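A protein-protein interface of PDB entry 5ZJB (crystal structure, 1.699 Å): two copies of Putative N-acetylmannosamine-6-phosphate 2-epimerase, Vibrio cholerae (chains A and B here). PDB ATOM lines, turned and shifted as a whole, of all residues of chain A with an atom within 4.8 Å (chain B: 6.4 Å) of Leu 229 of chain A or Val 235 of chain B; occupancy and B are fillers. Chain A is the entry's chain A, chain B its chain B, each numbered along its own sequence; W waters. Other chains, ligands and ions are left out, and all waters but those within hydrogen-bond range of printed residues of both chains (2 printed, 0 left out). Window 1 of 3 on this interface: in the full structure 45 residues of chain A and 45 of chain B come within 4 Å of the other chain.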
ATOM      1  N   THR A  36     -27.422  28.309  -3.530  1.00  0.00           N
ATOM      2  CA  THR A  36     -27.613  28.010  -4.944  1.00  0.00           C
ATOM      3  C   THR A  36     -27.586  26.499  -5.128  1.00  0.00           C
ATOM      4  O   THR A  36     -26.601  25.850  -4.772  1.00  0.00           O
ATOM      5  CB  THR A  36     -26.522  28.658  -5.794  1.00  0.00           C
ATOM      6  OG1 THR A  36     -26.608  30.079  -5.648  1.00  0.00           O
ATOM      7  CG2 THR A  36     -26.702  28.285  -7.276  1.00  0.00           C
ATOM      8  N   VAL A  38     -27.368  23.475  -7.749  1.00  0.00           N
ATOM      9  CA  VAL A  38     -26.812  23.339  -9.094  1.00  0.00           C
ATOM     10  C   VAL A  38     -27.572  22.255  -9.840  1.00  0.00           C
ATOM     11  O   VAL A  38     -27.537  21.077  -9.457  1.00  0.00           O
ATOM     12  CB  VAL A  38     -25.311  23.035  -9.050  1.00  0.00           C
ATOM     13  CG1 VAL A  38     -24.740  23.049 -10.473  1.00  0.00           C
ATOM     14  CG2 VAL A  38     -24.594  24.045  -8.166  1.00  0.00           C
ATOM     15  N   VAL A 225     -30.012  26.879 -10.235  1.00  0.00           N
ATOM     16  CA  VAL A 225     -29.394  27.432 -11.439  1.00  0.00           C
ATOM     17  C   VAL A 225     -28.882  26.283 -12.300  1.00  0.00           C
ATOM     18  O   VAL A 225     -28.140  25.417 -11.817  1.00  0.00           O
ATOM     19  CB  VAL A 225     -28.252  28.391 -11.076  1.00  0.00           C
ATOM     20  CG1 VAL A 225     -27.552  28.921 -12.343  1.00  0.00           C
ATOM     21  CG2 VAL A 225     -28.792  29.542 -10.236  1.00  0.00           C
ATOM     22  N   GLY A 226     -29.248  26.298 -13.582  1.00  0.00           N
ATOM     23  CA  GLY A 226     -28.804  25.280 -14.515  1.00  0.00           C
ATOM     24  C   GLY A 226     -27.911  25.848 -15.602  1.00  0.00           C
ATOM     25  O   GLY A 226     -26.692  25.798 -15.475  1.00  0.00           O
ATOM     26  N   SER A 227     -28.516  26.424 -16.645  1.00  0.00           N
ATOM     27  CA  SER A 227     -27.768  26.794 -17.851  1.00  0.00           C
ATOM     28  C   SER A 227     -26.502  27.585 -17.530  1.00  0.00           C
ATOM     29  O   SER A 227     -25.422  27.300 -18.069  1.00  0.00           O
ATOM     30  CB  SER A 227     -28.668  27.607 -18.782  1.00  0.00           C
ATOM     31  OG  SER A 227     -29.579  26.771 -19.478  1.00  0.00           O
ATOM     32  N   ALA A 228     -26.621  28.600 -16.673  1.00  0.00           N
ATOM     33  CA  ALA A 228     -25.497  29.497 -16.419  1.00  0.00           C
ATOM     34  C   ALA A 228     -24.296  28.771 -15.827  1.00  0.00           C
ATOM     35  O   ALA A 228     -23.161  29.255 -15.948  1.00  0.00           O
ATOM     36  CB  ALA A 228     -25.942  30.643 -15.500  1.00  0.00           C
ATOM     37  N   LEU A 229     -24.510  27.614 -15.202  1.00  0.00           N
ATOM     38  CA  LEU A 229     -23.431  26.821 -14.635  1.00  0.00           C
ATOM     39  C   LEU A 229     -23.077  25.590 -15.460  1.00  0.00           C
ATOM     40  O   LEU A 229     -21.900  25.247 -15.560  1.00  0.00           O
ATOM     41  CB  LEU A 229     -23.789  26.382 -13.204  1.00  0.00           C
ATOM     42  CG  LEU A 229     -23.819  27.464 -12.117  1.00  0.00           C
ATOM     43  CD1 LEU A 229     -24.457  26.935 -10.843  1.00  0.00           C
ATOM     44  CD2 LEU A 229     -22.403  27.897 -11.812  1.00  0.00           C
ATOM     45  N   THR A 230     -24.056  24.890 -16.045  1.00  0.00           N
ATOM     46  CA  THR A 230     -23.789  23.554 -16.563  1.00  0.00           C
ATOM     47  C   THR A 230     -24.198  23.346 -18.019  1.00  0.00           C
ATOM     48  O   THR A 230     -24.189  22.201 -18.481  1.00  0.00           O
ATOM     49  CB  THR A 230     -24.460  22.489 -15.680  1.00  0.00           C
ATOM     50  OG1 THR A 230     -25.868  22.714 -15.673  1.00  0.00           O
ATOM     51  CG2 THR A 230     -23.914  22.560 -14.239  1.00  0.00           C
ATOM     52  N   ARG A 231     -24.513  24.405 -18.777  1.00  0.00           N
ATOM     53  CA  ARG A 231     -24.712  24.288 -20.228  1.00  0.00           C
ATOM     54  C   ARG A 231     -23.667  25.157 -20.924  1.00  0.00           C
ATOM     55  O   ARG A 231     -23.951  26.305 -21.282  1.00  0.00           O
ATOM     56  CB  ARG A 231     -26.136  24.681 -20.655  1.00  0.00           C
ATOM     57  CG  ARG A 231     -27.202  23.623 -20.269  1.00  0.00           C
ATOM     58  CD  ARG A 231     -28.571  23.911 -20.882  1.00  0.00           C
ATOM     59  NE  ARG A 231     -29.533  22.856 -20.510  1.00  0.00           N
ATOM     60  CZ  ARG A 231     -30.470  23.020 -19.592  1.00  0.00           C
ATOM     61  NH1 ARG A 231     -30.600  24.203 -18.987  1.00  0.00           N
ATOM     62  NH2 ARG A 231     -31.298  22.008 -19.293  1.00  0.00           N
ATOM     63  N   SER B 227     -12.469  31.619 -16.836  1.00  0.00           N
ATOM     64  CA  SER B 227     -13.196  31.183 -15.638  1.00  0.00           C
ATOM     65  C   SER B 227     -14.705  31.144 -15.854  1.00  0.00           C
ATOM     66  O   SER B 227     -15.364  30.142 -15.538  1.00  0.00           O
ATOM     67  CB  SER B 227     -12.862  32.100 -14.462  1.00  0.00           C
ATOM     68  OG  SER B 227     -11.513  31.974 -14.059  1.00  0.00           O
ATOM     69  N   ALA B 228     -15.285  32.241 -16.356  1.00  0.00           N
ATOM     70  CA  ALA B 228     -16.744  32.336 -16.436  1.00  0.00           C
ATOM     71  C   ALA B 228     -17.354  31.245 -17.310  1.00  0.00           C
ATOM     72  O   ALA B 228     -18.558  30.977 -17.196  1.00  0.00           O
ATOM     73  CB  ALA B 228     -17.171  33.710 -16.974  1.00  0.00           C
ATOM     74  N   LEU B 229     -16.567  30.635 -18.198  1.00  0.00           N
ATOM     75  CA  LEU B 229     -17.029  29.536 -19.045  1.00  0.00           C
ATOM     76  C   LEU B 229     -16.511  28.172 -18.619  1.00  0.00           C
ATOM     77  O   LEU B 229     -17.239  27.178 -18.747  1.00  0.00           O
ATOM     78  CB  LEU B 229     -16.619  29.784 -20.512  1.00  0.00           C
ATOM     79  CG  LEU B 229     -17.377  30.905 -21.229  1.00  0.00           C
ATOM     80  CD1 LEU B 229     -16.606  31.398 -22.454  1.00  0.00           C
ATOM     81  CD2 LEU B 229     -18.759  30.446 -21.665  1.00  0.00           C
ATOM     82  N   THR B 230     -15.265  28.054 -18.154  1.00  0.00           N
ATOM     83  CA  THR B 230     -14.681  26.723 -18.014  1.00  0.00           C
ATOM     84  C   THR B 230     -14.084  26.441 -16.643  1.00  0.00           C
ATOM     85  O   THR B 230     -13.367  25.437 -16.504  1.00  0.00           O
ATOM     86  CB  THR B 230     -13.606  26.485 -19.083  1.00  0.00           C
ATOM     87  OG1 THR B 230     -12.608  27.501 -18.950  1.00  0.00           O
ATOM     88  CG2 THR B 230     -14.234  26.533 -20.476  1.00  0.00           C
ATOM     89  N   ARG B 231     -14.381  27.255 -15.621  1.00  0.00           N
ATOM     90  CA  ARG B 231     -14.038  26.917 -14.235  1.00  0.00           C
ATOM     91  C   ARG B 231     -15.338  26.809 -13.443  1.00  0.00           C
ATOM     92  O   ARG B 231     -15.770  27.764 -12.794  1.00  0.00           O
ATOM     93  CB  ARG B 231     -13.075  27.933 -13.620  1.00  0.00           C
ATOM     94  CG  ARG B 231     -11.653  27.833 -14.222  1.00  0.00           C
ATOM     95  CD  ARG B 231     -10.637  28.642 -13.418  1.00  0.00           C
ATOM     96  NE  ARG B 231      -9.299  28.477 -13.978  1.00  0.00           N
ATOM     97  CZ  ARG B 231      -8.703  29.389 -14.739  1.00  0.00           C
ATOM     98  NH1 ARG B 231      -9.318  30.537 -15.006  1.00  0.00           N
ATOM     99  NH2 ARG B 231      -7.486  29.155 -15.223  1.00  0.00           N
ATOM    100  N   LEU B 232     -15.948  25.614 -13.475  1.00  0.00           N
ATOM    101  CA  LEU B 232     -17.267  25.453 -12.872  1.00  0.00           C
ATOM    102  C   LEU B 232     -17.245  25.800 -11.385  1.00  0.00           C
ATOM    103  O   LEU B 232     -18.199  26.394 -10.868  1.00  0.00           O
ATOM    104  CB  LEU B 232     -17.758  24.020 -13.098  1.00  0.00           C
ATOM    105  CG  LEU B 232     -19.053  23.630 -12.376  1.00  0.00           C
ATOM    106  CD1 LEU B 232     -20.194  24.508 -12.805  1.00  0.00           C
ATOM    107  CD2 LEU B 232     -19.343  22.165 -12.687  1.00  0.00           C
ATOM    108  N   GLU B 233     -16.174  25.423 -10.679  1.00  0.00           N
ATOM    109  CA  GLU B 233     -16.094  25.691  -9.243  1.00  0.00           C
ATOM    110  C   GLU B 233     -16.091  27.184  -8.959  1.00  0.00           C
ATOM    111  O   GLU B 233     -16.648  27.639  -7.958  1.00  0.00           O
ATOM    112  CB  GLU B 233     -14.838  25.057  -8.646  1.00  0.00           C
ATOM    113  CG  GLU B 233     -14.811  23.532  -8.649  1.00  0.00           C
ATOM    114  CD  GLU B 233     -14.156  22.944  -9.881  1.00  0.00           C
ATOM    115  OE1 GLU B 233     -14.195  23.578 -10.966  1.00  0.00           O
ATOM    116  OE2 GLU B 233     -13.581  21.842  -9.761  1.00  0.00           O
ATOM    117  N   VAL B 234     -15.434  27.960  -9.818  1.00  0.00           N
ATOM    118  CA  VAL B 234     -15.369  29.399  -9.614  1.00  0.00           C
ATOM    119  C   VAL B 234     -16.743  30.030  -9.790  1.00  0.00           C
ATOM    120  O   VAL B 234     -17.190  30.828  -8.959  1.00  0.00           O
ATOM    121  CB  VAL B 234     -14.339  30.010 -10.578  1.00  0.00           C
ATOM    122  CG1 VAL B 234     -14.352  31.526 -10.463  1.00  0.00           C
ATOM    123  CG2 VAL B 234     -12.960  29.430 -10.282  1.00  0.00           C
ATOM    124  N   VAL B 235     -17.441  29.676 -10.870  1.00  0.00           N
ATOM    125  CA  VAL B 235     -18.745  30.264 -11.132  1.00  0.00           C
ATOM    126  C   VAL B 235     -19.736  29.853 -10.048  1.00  0.00           C
ATOM    127  O   VAL B 235     -20.589  30.644  -9.629  1.00  0.00           O
ATOM    128  CB  VAL B 235     -19.236  29.867 -12.534  1.00  0.00           C
ATOM    129  CG1 VAL B 235     -20.502  30.603 -12.871  1.00  0.00           C
ATOM    130  CG2 VAL B 235     -18.149  30.181 -13.592  1.00  0.00           C
ATOM    131  N   THR B 236     -19.652  28.599  -9.604  1.00  0.00           N
ATOM    132  CA  THR B 236     -20.485  28.157  -8.490  1.00  0.00           C
ATOM    133  C   THR B 236     -20.307  29.061  -7.270  1.00  0.00           C
ATOM    134  O   THR B 236     -21.286  29.496  -6.656  1.00  0.00           O
ATOM    135  CB  THR B 236     -20.154  26.706  -8.145  1.00  0.00           C
ATOM    136  OG1 THR B 236     -20.387  25.876  -9.292  1.00  0.00           O
ATOM    137  CG2 THR B 236     -21.028  26.224  -6.983  1.00  0.00           C
ATOM    138  N   GLN B 237     -19.063  29.377  -6.922  1.00  0.00           N
ATOM    139  CA  GLN B 237     -18.840  30.239  -5.766  1.00  0.00           C
ATOM    140  C   GLN B 237     -19.329  31.664  -6.013  1.00  0.00           C
ATOM    141  O   GLN B 237     -19.797  32.319  -5.075  1.00  0.00           O
ATOM    142  CB  GLN B 237     -17.366  30.216  -5.387  1.00  0.00           C
ATOM    143  CG  GLN B 237     -16.915  28.832  -4.953  1.00  0.00           C
ATOM    144  CD  GLN B 237     -15.565  28.829  -4.288  1.00  0.00           C
ATOM    145  OE1 GLN B 237     -14.827  29.810  -4.357  1.00  0.00           O
ATOM    146  NE2 GLN B 237     -15.235  27.727  -3.625  1.00  0.00           N
ATOM    147  N   TRP B 238     -19.239  32.158  -7.256  1.00  0.00           N
ATOM    148  CA  TRP B 238     -19.825  33.457  -7.576  1.00  0.00           C
ATOM    149  C   TRP B 238     -21.306  33.482  -7.225  1.00  0.00           C
ATOM    150  O   TRP B 238     -21.805  34.444  -6.625  1.00  0.00           O
ATOM    151  CB  TRP B 238     -19.649  33.779  -9.055  1.00  0.00           C
ATOM    152  CG  TRP B 238     -18.249  34.054  -9.492  1.00  0.00           C
ATOM    153  CD1 TRP B 238     -17.152  34.272  -8.702  1.00  0.00           C
ATOM    154  CD2 TRP B 238     -17.800  34.152 -10.843  1.00  0.00           C
ATOM    155  NE1 TRP B 238     -16.036  34.501  -9.493  1.00  0.00           N
ATOM    156  CE2 TRP B 238     -16.415  34.430 -10.809  1.00  0.00           C
ATOM    157  CE3 TRP B 238     -18.435  34.030 -12.085  1.00  0.00           C
ATOM    158  CZ2 TRP B 238     -15.662  34.587 -11.969  1.00  0.00           C
ATOM    159  CZ3 TRP B 238     -17.683  34.189 -13.234  1.00  0.00           C
ATOM    160  CH2 TRP B 238     -16.316  34.465 -13.166  1.00  0.00           C
ATOM    161  N   PHE B 239     -22.031  32.425  -7.611  1.00  0.00           N
ATOM    162  CA  PHE B 239     -23.456  32.368  -7.318  1.00  0.00           C
ATOM    163  C   PHE B 239     -23.704  32.258  -5.820  1.00  0.00           C
ATOM    164  O   PHE B 239     -24.524  33.002  -5.263  1.00  0.00           O
ATOM    165  CB  PHE B 239     -24.098  31.203  -8.070  1.00  0.00           C
ATOM    166  CG  PHE B 239     -24.538  31.564  -9.456  1.00  0.00           C
ATOM    167  CD1 PHE B 239     -23.641  31.495 -10.509  1.00  0.00           C
ATOM    168  CD2 PHE B 239     -25.835  31.987  -9.705  1.00  0.00           C
ATOM    169  CE1 PHE B 239     -24.033  31.837 -11.790  1.00  0.00           C
ATOM    170  CE2 PHE B 239     -26.245  32.322 -10.976  1.00  0.00           C
ATOM    171  CZ  PHE B 239     -25.326  32.258 -12.032  1.00  0.00           C
ATOM    172  N   ASN B 240     -22.999  31.348  -5.143  1.00  0.00           N
ATOM    173  CA  ASN B 240     -23.263  31.146  -3.719  1.00  0.00           C
ATOM    174  C   ASN B 240     -22.851  32.369  -2.909  1.00  0.00           C
ATOM    175  O   ASN B 240     -23.505  32.712  -1.918  1.00  0.00           O
ATOM    176  CB  ASN B 240     -22.549  29.905  -3.205  1.00  0.00           C
ATOM    177  CG  ASN B 240     -23.487  28.718  -3.059  1.00  0.00           C
ATOM    178  OD1 ASN B 240     -24.711  28.883  -2.952  1.00  0.00           O
ATOM    179  ND2 ASN B 240     -22.920  27.520  -3.043  1.00  0.00           N
HETATM  180  O   HOH W   1     -20.522  28.965 -16.752  1.00  0.00           O
HETATM  181  O   HOH W   2     -25.160  25.614  -2.409  1.00  0.00           O
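The backbone NH of Thr 36 of chain A lies within hydrogen-bond range of the side-chain amide oxygen of Asn 240 of chain B (2.8 Å).
The backbone carbonyl oxygen (O) of Leu 232 of chain B lies within hydrogen-bond range of the side-chain hydroxyl (OG1) of Thr 236 of chain B (2.7 Å).
Phe 239 of chain B touches Thr 36 of chain A.
CG2 of Val 225 of chain A touches CE2 of Phe 239 of chain B (3.8 Å).
CZ of Phe 239 of chain B touches CB of Ala 228 of chain A (3.9 Å).
Leu 229 of chain A touches Leu 232 of chain B (O to CD1, 3.3 Å).
Leu 229 of chain A touches Val 235 of chain B.
Leu 229 of chain A touches Thr 236 of chain B.
Leu 229 of chain A touches just these residues of chain B: Leu 232, Val 235 and Thr 236.
Of the printed residues of chain B, Ala 228 of chain A touches Phe 239 (3.9 Å).
Of the printed residues of chain B, Val 225 of chain A touches Phe 239.
Val 38 of chain A touches none of the printed residues of chain B.
The nearest residue of chain B that does not touch Leu 229 of chain A is Phe 239 of chain B (4.02 Å).
The nearest printed residue of chain A that does not touch Leu 232 of chain B is Thr 230 of chain A (4.4 Å).
Of the 9 printed residues of chain A, 4 touch a printed residue of chain B.
Printed residues of chain A that touch a printed residue of chain B: Thr 36, Val 225, Ala 228 and Leu 229.
Of the 14 printed residues of chain B, 5 touch a printed residue of chain A.
Hydrophobic or aromatic side chains of chain B that line the printed part of chain A: Leu 232, Val 235 and Phe 239.
Among the printed residues, no Asp or Glu carboxylate lies within 4 Å of a Lys or Arg side-chain nitrogen of the other chain.
5 positions are printed for both chains.
Of the 7 pairs that touch across the chains among the printed residues, none has its exchanged pair printed and touching as well.
Water W1 lies within hydrogen-bond range of the backbone carbonyl oxygen (O) of Ala 228 of chain A (2.8 Å) and the backbone carbonyl oxygen (O) of Ala 228 of chain B (2.8 Å).
Water W2 bridges the backbone carbonyl oxygen (O) of Thr 36 of chain A (2.8 Å) and the side-chain amide nitrogen (ND2) of Asn 240 of chain B (3.0 Å).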
